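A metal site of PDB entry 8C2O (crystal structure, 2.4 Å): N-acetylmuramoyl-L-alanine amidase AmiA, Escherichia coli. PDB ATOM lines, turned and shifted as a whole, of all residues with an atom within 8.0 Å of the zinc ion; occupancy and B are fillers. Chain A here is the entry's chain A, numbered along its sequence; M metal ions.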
ATOM      1  N   PRO A  30     -21.635   6.439  22.774  1.00  0.00           N
ATOM      2  CA  PRO A  30     -22.145   5.777  21.589  1.00  0.00           C
ATOM      3  C   PRO A  30     -23.225   6.660  20.970  1.00  0.00           C
ATOM      4  O   PRO A  30     -24.253   6.925  21.579  1.00  0.00           O
ATOM      5  CB  PRO A  30     -22.667   4.434  22.083  1.00  0.00           C
ATOM      6  CG  PRO A  30     -22.377   4.417  23.582  1.00  0.00           C
ATOM      7  CD  PRO A  30     -22.148   5.841  24.000  1.00  0.00           C
ATOM      8  N   GLY A  31     -22.974   7.117  19.749  1.00  0.00           N
ATOM      9  CA  GLY A  31     -23.793   8.126  19.120  1.00  0.00           C
ATOM     10  C   GLY A  31     -25.192   7.586  18.881  1.00  0.00           C
ATOM     11  O   GLY A  31     -25.382   6.373  18.822  1.00  0.00           O
ATOM     12  N   HIS A  32     -26.159   8.502  18.785  1.00  0.00           N
ATOM     13  CA  HIS A  32     -27.529   8.142  18.492  1.00  0.00           C
ATOM     14  C   HIS A  32     -28.081   7.262  19.620  1.00  0.00           C
ATOM     15  O   HIS A  32     -27.525   7.237  20.725  1.00  0.00           O
ATOM     16  CB  HIS A  32     -27.608   7.612  17.065  1.00  0.00           C
ATOM     17  CG  HIS A  32     -26.828   8.466  16.123  1.00  0.00           C
ATOM     18  ND1 HIS A  32     -27.185   9.748  15.759  1.00  0.00           N
ATOM     19  CD2 HIS A  32     -25.634   8.220  15.516  1.00  0.00           C
ATOM     20  CE1 HIS A  32     -26.250  10.250  14.954  1.00  0.00           C
ATOM     21  NE2 HIS A  32     -25.297   9.355  14.817  1.00  0.00           N
ATOM     22  N   ASP A  36     -33.490   7.896  17.522  1.00  0.00           N
ATOM     23  CA  ASP A  36     -32.436   8.287  16.586  1.00  0.00           C
ATOM     24  C   ASP A  36     -31.634   7.063  16.196  1.00  0.00           C
ATOM     25  O   ASP A  36     -30.774   6.615  16.944  1.00  0.00           O
ATOM     26  CB  ASP A  36     -31.555   9.386  17.160  1.00  0.00           C
ATOM     27  CG  ASP A  36     -30.472   9.878  16.205  1.00  0.00           C
ATOM     28  OD1 ASP A  36     -30.589   9.593  14.987  1.00  0.00           O
ATOM     29  OD2 ASP A  36     -29.525  10.528  16.688  1.00  0.00           O
ATOM     30  N   THR A  37     -31.934   6.505  15.020  1.00  0.00           N
ATOM     31  CA  THR A  37     -31.242   5.358  14.469  1.00  0.00           C
ATOM     32  C   THR A  37     -29.805   5.694  14.060  1.00  0.00           C
ATOM     33  O   THR A  37     -29.018   4.784  13.871  1.00  0.00           O
ATOM     34  CB  THR A  37     -31.899   4.851  13.189  1.00  0.00           C
ATOM     35  OG1 THR A  37     -31.853   5.903  12.238  1.00  0.00           O
ATOM     36  CG2 THR A  37     -33.338   4.434  13.356  1.00  0.00           C
ATOM     37  N   GLY A  38     -29.458   6.979  13.937  1.00  0.00           N
ATOM     38  CA  GLY A  38     -28.314   7.393  13.155  1.00  0.00           C
ATOM     39  C   GLY A  38     -28.485   7.068  11.675  1.00  0.00           C
ATOM     40  O   GLY A  38     -29.584   6.839  11.219  1.00  0.00           O
ATOM     41  N   ALA A  39     -27.376   7.028  10.934  1.00  0.00           N
ATOM     42  CA  ALA A  39     -27.422   6.661   9.524  1.00  0.00           C
ATOM     43  C   ALA A  39     -27.877   5.224   9.384  1.00  0.00           C
ATOM     44  O   ALA A  39     -27.629   4.439  10.291  1.00  0.00           O
ATOM     45  CB  ALA A  39     -26.080   6.854   8.879  1.00  0.00           C
ATOM     46  N   GLU A  47     -26.672   2.691  12.412  1.00  0.00           N
ATOM     47  CA  GLU A  47     -25.505   3.221  13.094  1.00  0.00           C
ATOM     48  C   GLU A  47     -25.586   2.982  14.603  1.00  0.00           C
ATOM     49  O   GLU A  47     -24.602   2.570  15.192  1.00  0.00           O
ATOM     50  CB  GLU A  47     -25.376   4.704  12.773  1.00  0.00           C
ATOM     51  CG  GLU A  47     -24.152   5.383  13.357  1.00  0.00           C
ATOM     52  CD  GLU A  47     -24.109   6.871  13.040  1.00  0.00           C
ATOM     53  OE1 GLU A  47     -25.055   7.369  12.383  1.00  0.00           O
ATOM     54  OE2 GLU A  47     -23.142   7.523  13.435  1.00  0.00           O
ATOM     55  N   LYS A  48     -26.760   3.230  15.219  1.00  0.00           N
ATOM     56  CA  LYS A  48     -26.872   3.281  16.668  1.00  0.00           C
ATOM     57  C   LYS A  48     -26.544   1.934  17.299  1.00  0.00           C
ATOM     58  O   LYS A  48     -26.006   1.895  18.414  1.00  0.00           O
ATOM     59  CB  LYS A  48     -28.261   3.760  17.098  1.00  0.00           C
ATOM     60  CG  LYS A  48     -29.396   2.781  16.752  1.00  0.00           C
ATOM     61  CD  LYS A  48     -30.713   3.135  17.370  1.00  0.00           C
ATOM     62  CE  LYS A  48     -31.780   2.159  16.986  1.00  0.00           C
ATOM     63  NZ  LYS A  48     -32.974   2.277  17.842  1.00  0.00           N
ATOM     64  N   VAL A  51     -22.550   1.206  16.845  1.00  0.00           N
ATOM     65  CA  VAL A  51     -21.643   2.024  17.630  1.00  0.00           C
ATOM     66  C   VAL A  51     -21.776   1.683  19.111  1.00  0.00           C
ATOM     67  O   VAL A  51     -20.818   1.891  19.856  1.00  0.00           O
ATOM     68  CB  VAL A  51     -21.813   3.535  17.365  1.00  0.00           C
ATOM     69  CG1 VAL A  51     -21.500   3.838  15.907  1.00  0.00           C
ATOM     70  CG2 VAL A  51     -23.177   4.095  17.747  1.00  0.00           C
ATOM     71  N   SER A  98     -16.878  10.478  21.297  1.00  0.00           N
ATOM     72  CA  SER A  98     -18.092  10.055  20.653  1.00  0.00           C
ATOM     73  C   SER A  98     -17.769   9.096  19.497  1.00  0.00           C
ATOM     74  O   SER A  98     -16.887   9.361  18.688  1.00  0.00           O
ATOM     75  CB  SER A  98     -18.848  11.270  20.205  1.00  0.00           C
ATOM     76  OG  SER A  98     -20.249  11.005  20.058  1.00  0.00           O
ATOM     77  N   ILE A  99     -18.506   7.996  19.393  1.00  0.00           N
ATOM     78  CA  ILE A  99     -18.240   6.949  18.428  1.00  0.00           C
ATOM     79  C   ILE A  99     -19.446   6.822  17.499  1.00  0.00           C
ATOM     80  O   ILE A  99     -20.562   6.584  17.952  1.00  0.00           O
ATOM     81  CB  ILE A  99     -17.930   5.609  19.120  1.00  0.00           C
ATOM     82  CG1 ILE A  99     -16.675   5.739  19.986  1.00  0.00           C
ATOM     83  CG2 ILE A  99     -17.792   4.473  18.119  1.00  0.00           C
ATOM     84  CD1 ILE A  99     -16.497   4.547  20.872  1.00  0.00           C
ATOM     85  N   HIS A 100     -19.169   6.999  16.199  1.00  0.00           N
ATOM     86  CA  HIS A 100     -20.186   7.094  15.182  1.00  0.00           C
ATOM     87  C   HIS A 100     -19.795   6.178  14.029  1.00  0.00           C
ATOM     88  O   HIS A 100     -18.710   5.597  14.022  1.00  0.00           O
ATOM     89  CB  HIS A 100     -20.357   8.544  14.727  1.00  0.00           C
ATOM     90  CG  HIS A 100     -20.945   9.415  15.778  1.00  0.00           C
ATOM     91  ND1 HIS A 100     -22.282   9.762  15.776  1.00  0.00           N
ATOM     92  CD2 HIS A 100     -20.435   9.943  16.891  1.00  0.00           C
ATOM     93  CE1 HIS A 100     -22.519  10.507  16.841  1.00  0.00           C
ATOM     94  NE2 HIS A 100     -21.421  10.609  17.547  1.00  0.00           N
ATOM     95  N   ALA A 101     -20.691   6.120  13.067  1.00  0.00           N
ATOM     96  CA  ALA A 101     -20.521   5.410  11.809  1.00  0.00           C
ATOM     97  C   ALA A 101     -21.576   5.973  10.876  1.00  0.00           C
ATOM     98  O   ALA A 101     -22.564   5.306  10.549  1.00  0.00           O
ATOM     99  CB  ALA A 101     -20.705   3.922  11.983  1.00  0.00           C
ATOM    100  N   ASP A 102     -21.397   7.244  10.507  1.00  0.00           N
ATOM    101  CA  ASP A 102     -22.481   7.996   9.921  1.00  0.00           C
ATOM    102  C   ASP A 102     -22.443   7.886   8.389  1.00  0.00           C
ATOM    103  O   ASP A 102     -21.832   6.983   7.797  1.00  0.00           O
ATOM    104  CB  ASP A 102     -22.515   9.404  10.539  1.00  0.00           C
ATOM    105  CG  ASP A 102     -23.955   9.901  10.659  1.00  0.00           C
ATOM    106  OD1 ASP A 102     -24.643   9.993   9.603  1.00  0.00           O
ATOM    107  OD2 ASP A 102     -24.393  10.150  11.822  1.00  0.00           O
ATOM    108  N   GLY A 103     -23.179   8.788   7.717  1.00  0.00           N
ATOM    109  CA  GLY A 103     -23.466   8.592   6.315  1.00  0.00           C
ATOM    110  C   GLY A 103     -23.055   9.790   5.456  1.00  0.00           C
ATOM    111  O   GLY A 103     -22.952  10.908   5.948  1.00  0.00           O
ATOM    112  N   LEU A 130     -20.410  16.548   8.079  1.00  0.00           N
ATOM    113  CA  LEU A 130     -20.723  15.590   9.132  1.00  0.00           C
ATOM    114  C   LEU A 130     -21.064  16.334  10.434  1.00  0.00           C
ATOM    115  O   LEU A 130     -21.961  15.905  11.153  1.00  0.00           O
ATOM    116  CB  LEU A 130     -19.567  14.617   9.311  1.00  0.00           C
ATOM    117  CG  LEU A 130     -19.403  13.590   8.190  1.00  0.00           C
ATOM    118  CD1 LEU A 130     -18.163  12.730   8.433  1.00  0.00           C
ATOM    119  CD2 LEU A 130     -20.623  12.697   8.089  1.00  0.00           C
ATOM    120  N   ARG A 133     -24.713  17.161   9.873  1.00  0.00           N
ATOM    121  CA  ARG A 133     -25.516  15.960   9.985  1.00  0.00           C
ATOM    122  C   ARG A 133     -25.553  15.480  11.443  1.00  0.00           C
ATOM    123  O   ARG A 133     -26.620  15.168  11.965  1.00  0.00           O
ATOM    124  CB  ARG A 133     -24.938  14.920   9.028  1.00  0.00           C
ATOM    125  CG  ARG A 133     -25.801  13.681   8.849  1.00  0.00           C
ATOM    126  CD  ARG A 133     -25.186  12.690   7.866  1.00  0.00           C
ATOM    127  NE  ARG A 133     -26.058  11.524   7.650  1.00  0.00           N
ATOM    128  CZ  ARG A 133     -26.359  10.966   6.475  1.00  0.00           C
ATOM    129  NH1 ARG A 133     -25.844  11.437   5.343  1.00  0.00           N
ATOM    130  NH2 ARG A 133     -27.163   9.916   6.434  1.00  0.00           N
ATOM    131  N   GLU A 134     -24.389  15.415  12.123  1.00  0.00           N
ATOM    132  CA  GLU A 134     -24.379  14.898  13.477  1.00  0.00           C
ATOM    133  C   GLU A 134     -25.071  15.896  14.420  1.00  0.00           C
ATOM    134  O   GLU A 134     -25.759  15.521  15.363  1.00  0.00           O
ATOM    135  CB  GLU A 134     -22.965  14.618  14.017  1.00  0.00           C
ATOM    136  CG  GLU A 134     -22.174  13.551  13.311  1.00  0.00           C
ATOM    137  CD  GLU A 134     -22.616  12.110  13.468  1.00  0.00           C
ATOM    138  OE1 GLU A 134     -23.733  11.867  14.031  1.00  0.00           O
ATOM    139  OE2 GLU A 134     -21.832  11.217  12.958  1.00  0.00           O
ATOM    140  N   ASN A 135     -24.882  17.196  14.187  1.00  0.00           N
ATOM    141  CA  ASN A 135     -25.417  18.183  15.092  1.00  0.00           C
ATOM    142  C   ASN A 135     -26.940  18.234  15.045  1.00  0.00           C
ATOM    143  O   ASN A 135     -27.528  18.704  16.022  1.00  0.00           O
ATOM    144  CB  ASN A 135     -24.875  19.579  14.824  1.00  0.00           C
ATOM    145  CG  ASN A 135     -23.465  19.758  15.278  1.00  0.00           C
ATOM    146  OD1 ASN A 135     -22.910  18.951  16.034  1.00  0.00           O
ATOM    147  ND2 ASN A 135     -22.851  20.838  14.826  1.00  0.00           N
ATOM    148  N   ALA A 137     -28.926  15.684  15.049  1.00  0.00           N
ATOM    149  CA  ALA A 137     -29.511  14.520  15.721  1.00  0.00           C
ATOM    150  C   ALA A 137     -30.583  14.943  16.719  1.00  0.00           C
ATOM    151  O   ALA A 137     -31.544  14.211  16.915  1.00  0.00           O
ATOM    152  CB  ALA A 137     -28.426  13.739  16.417  1.00  0.00           C
ATOM    153  N   PHE A 195     -18.620  20.469  15.978  1.00  0.00           N
ATOM    154  CA  PHE A 195     -19.466  19.417  16.543  1.00  0.00           C
ATOM    155  C   PHE A 195     -19.946  19.821  17.952  1.00  0.00           C
ATOM    156  O   PHE A 195     -19.149  20.084  18.845  1.00  0.00           O
ATOM    157  CB  PHE A 195     -18.658  18.135  16.602  1.00  0.00           C
ATOM    158  CG  PHE A 195     -18.339  17.504  15.274  1.00  0.00           C
ATOM    159  CD1 PHE A 195     -19.215  16.611  14.683  1.00  0.00           C
ATOM    160  CD2 PHE A 195     -17.127  17.776  14.638  1.00  0.00           C
ATOM    161  CE1 PHE A 195     -18.913  16.027  13.458  1.00  0.00           C
ATOM    162  CE2 PHE A 195     -16.852  17.203  13.407  1.00  0.00           C
ATOM    163  CZ  PHE A 195     -17.743  16.332  12.822  1.00  0.00           C
ATOM    164  N   LEU A 207     -14.573  13.080  18.182  1.00  0.00           N
ATOM    165  CA  LEU A 207     -15.589  12.228  17.587  1.00  0.00           C
ATOM    166  C   LEU A 207     -14.910  11.332  16.557  1.00  0.00           C
ATOM    167  O   LEU A 207     -14.197  11.799  15.681  1.00  0.00           O
ATOM    168  CB  LEU A 207     -16.686  13.102  16.965  1.00  0.00           C
ATOM    169  CG  LEU A 207     -17.885  12.331  16.398  1.00  0.00           C
ATOM    170  CD1 LEU A 207     -19.165  13.166  16.472  1.00  0.00           C
ATOM    171  CD2 LEU A 207     -17.630  11.875  14.973  1.00  0.00           C
ATOM    172  N   VAL A 208     -15.140  10.029  16.675  1.00  0.00           N
ATOM    173  CA  VAL A 208     -14.545   9.039  15.824  1.00  0.00           C
ATOM    174  C   VAL A 208     -15.610   8.478  14.894  1.00  0.00           C
ATOM    175  O   VAL A 208     -16.625   7.974  15.359  1.00  0.00           O
ATOM    176  CB  VAL A 208     -13.920   7.902  16.630  1.00  0.00           C
ATOM    177  CG1 VAL A 208     -13.382   6.825  15.682  1.00  0.00           C
ATOM    178  CG2 VAL A 208     -12.812   8.376  17.535  1.00  0.00           C
ATOM    179  N   GLU A 209     -15.376   8.590  13.578  1.00  0.00           N
ATOM    180  CA  GLU A 209     -16.188   7.891  12.607  1.00  0.00           C
ATOM    181  C   GLU A 209     -15.446   6.617  12.294  1.00  0.00           C
ATOM    182  O   GLU A 209     -14.312   6.677  11.846  1.00  0.00           O
ATOM    183  CB  GLU A 209     -16.426   8.711  11.341  1.00  0.00           C
ATOM    184  CG  GLU A 209     -17.167  10.015  11.583  1.00  0.00           C
ATOM    185  CD  GLU A 209     -18.655   9.880  11.731  1.00  0.00           C
ATOM    186  OE1 GLU A 209     -19.126   8.733  11.659  1.00  0.00           O
ATOM    187  OE2 GLU A 209     -19.341  10.926  11.910  1.00  0.00           O
ATOM    188  N   SER A 211     -16.393   4.317  10.165  1.00  0.00           N
ATOM    189  CA  SER A 211     -16.585   4.068   8.738  1.00  0.00           C
ATOM    190  C   SER A 211     -17.777   4.925   8.304  1.00  0.00           C
ATOM    191  O   SER A 211     -18.315   5.715   9.103  1.00  0.00           O
ATOM    192  CB  SER A 211     -16.851   2.600   8.430  1.00  0.00           C
ATOM    193  OG  SER A 211     -15.661   1.818   8.456  1.00  0.00           O
HETATM  194 ZN    ZN M   1     -23.388   9.615  13.763  1.00  0.00          ZN
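The backbone NH (N) of Ala 39 is in hydrogen-bond range of the side-chain carboxylate (OE1) of Glu 47 (2.8 Å). N of Glu 47 is in hydrogen-bond range of O of Thr 37, at 3.5 Å. A ring nitrogen (ND1) of His 32 lies within hydrogen-bond range of the side-chain carboxylate (OD2) of Asp 36 (2.6 Å). The backbone NH of Asp 102 lies within hydrogen-bond range of the side-chain carboxylate of Glu 209. The side-chain carboxylate (OD1) of Asp 102 is in salt-bridge range of the guanidinium group (NE) of Arg 133, at 2.9 Å. The side-chain carboxylate of Glu 134 lies close to the side-chain carboxylate of Glu 209. The backbone carbonyl oxygen (O) of Val 208 lies within hydrogen-bond range of the backbone NH (N) of His 100, at 2.9 Å. A ring nitrogen (NE2) of His 100 lies within hydrogen-bond range of the side-chain hydroxyl of Ser 98 (2.8 Å).
The zinc ion is bound by OE2 of Glu 47 (2.1 Å). The zinc ion is bound by NE2 of His 32, 2.2 Å away. The zinc ion is bound by OD2 of Asp 102, 2.3 Å away. The side-chain carboxylate (OE1) of Glu 134 binds the zinc ion (2.3 Å). ND1 of His 100 is bound to the zinc ion, at 2.3 Å. OE2 of Glu 134 is bound to the zinc ion (2.4 Å).
Within 4 Å of the zinc ion: His 32, Glu 47, His 100, Asp 102 and Glu 134.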
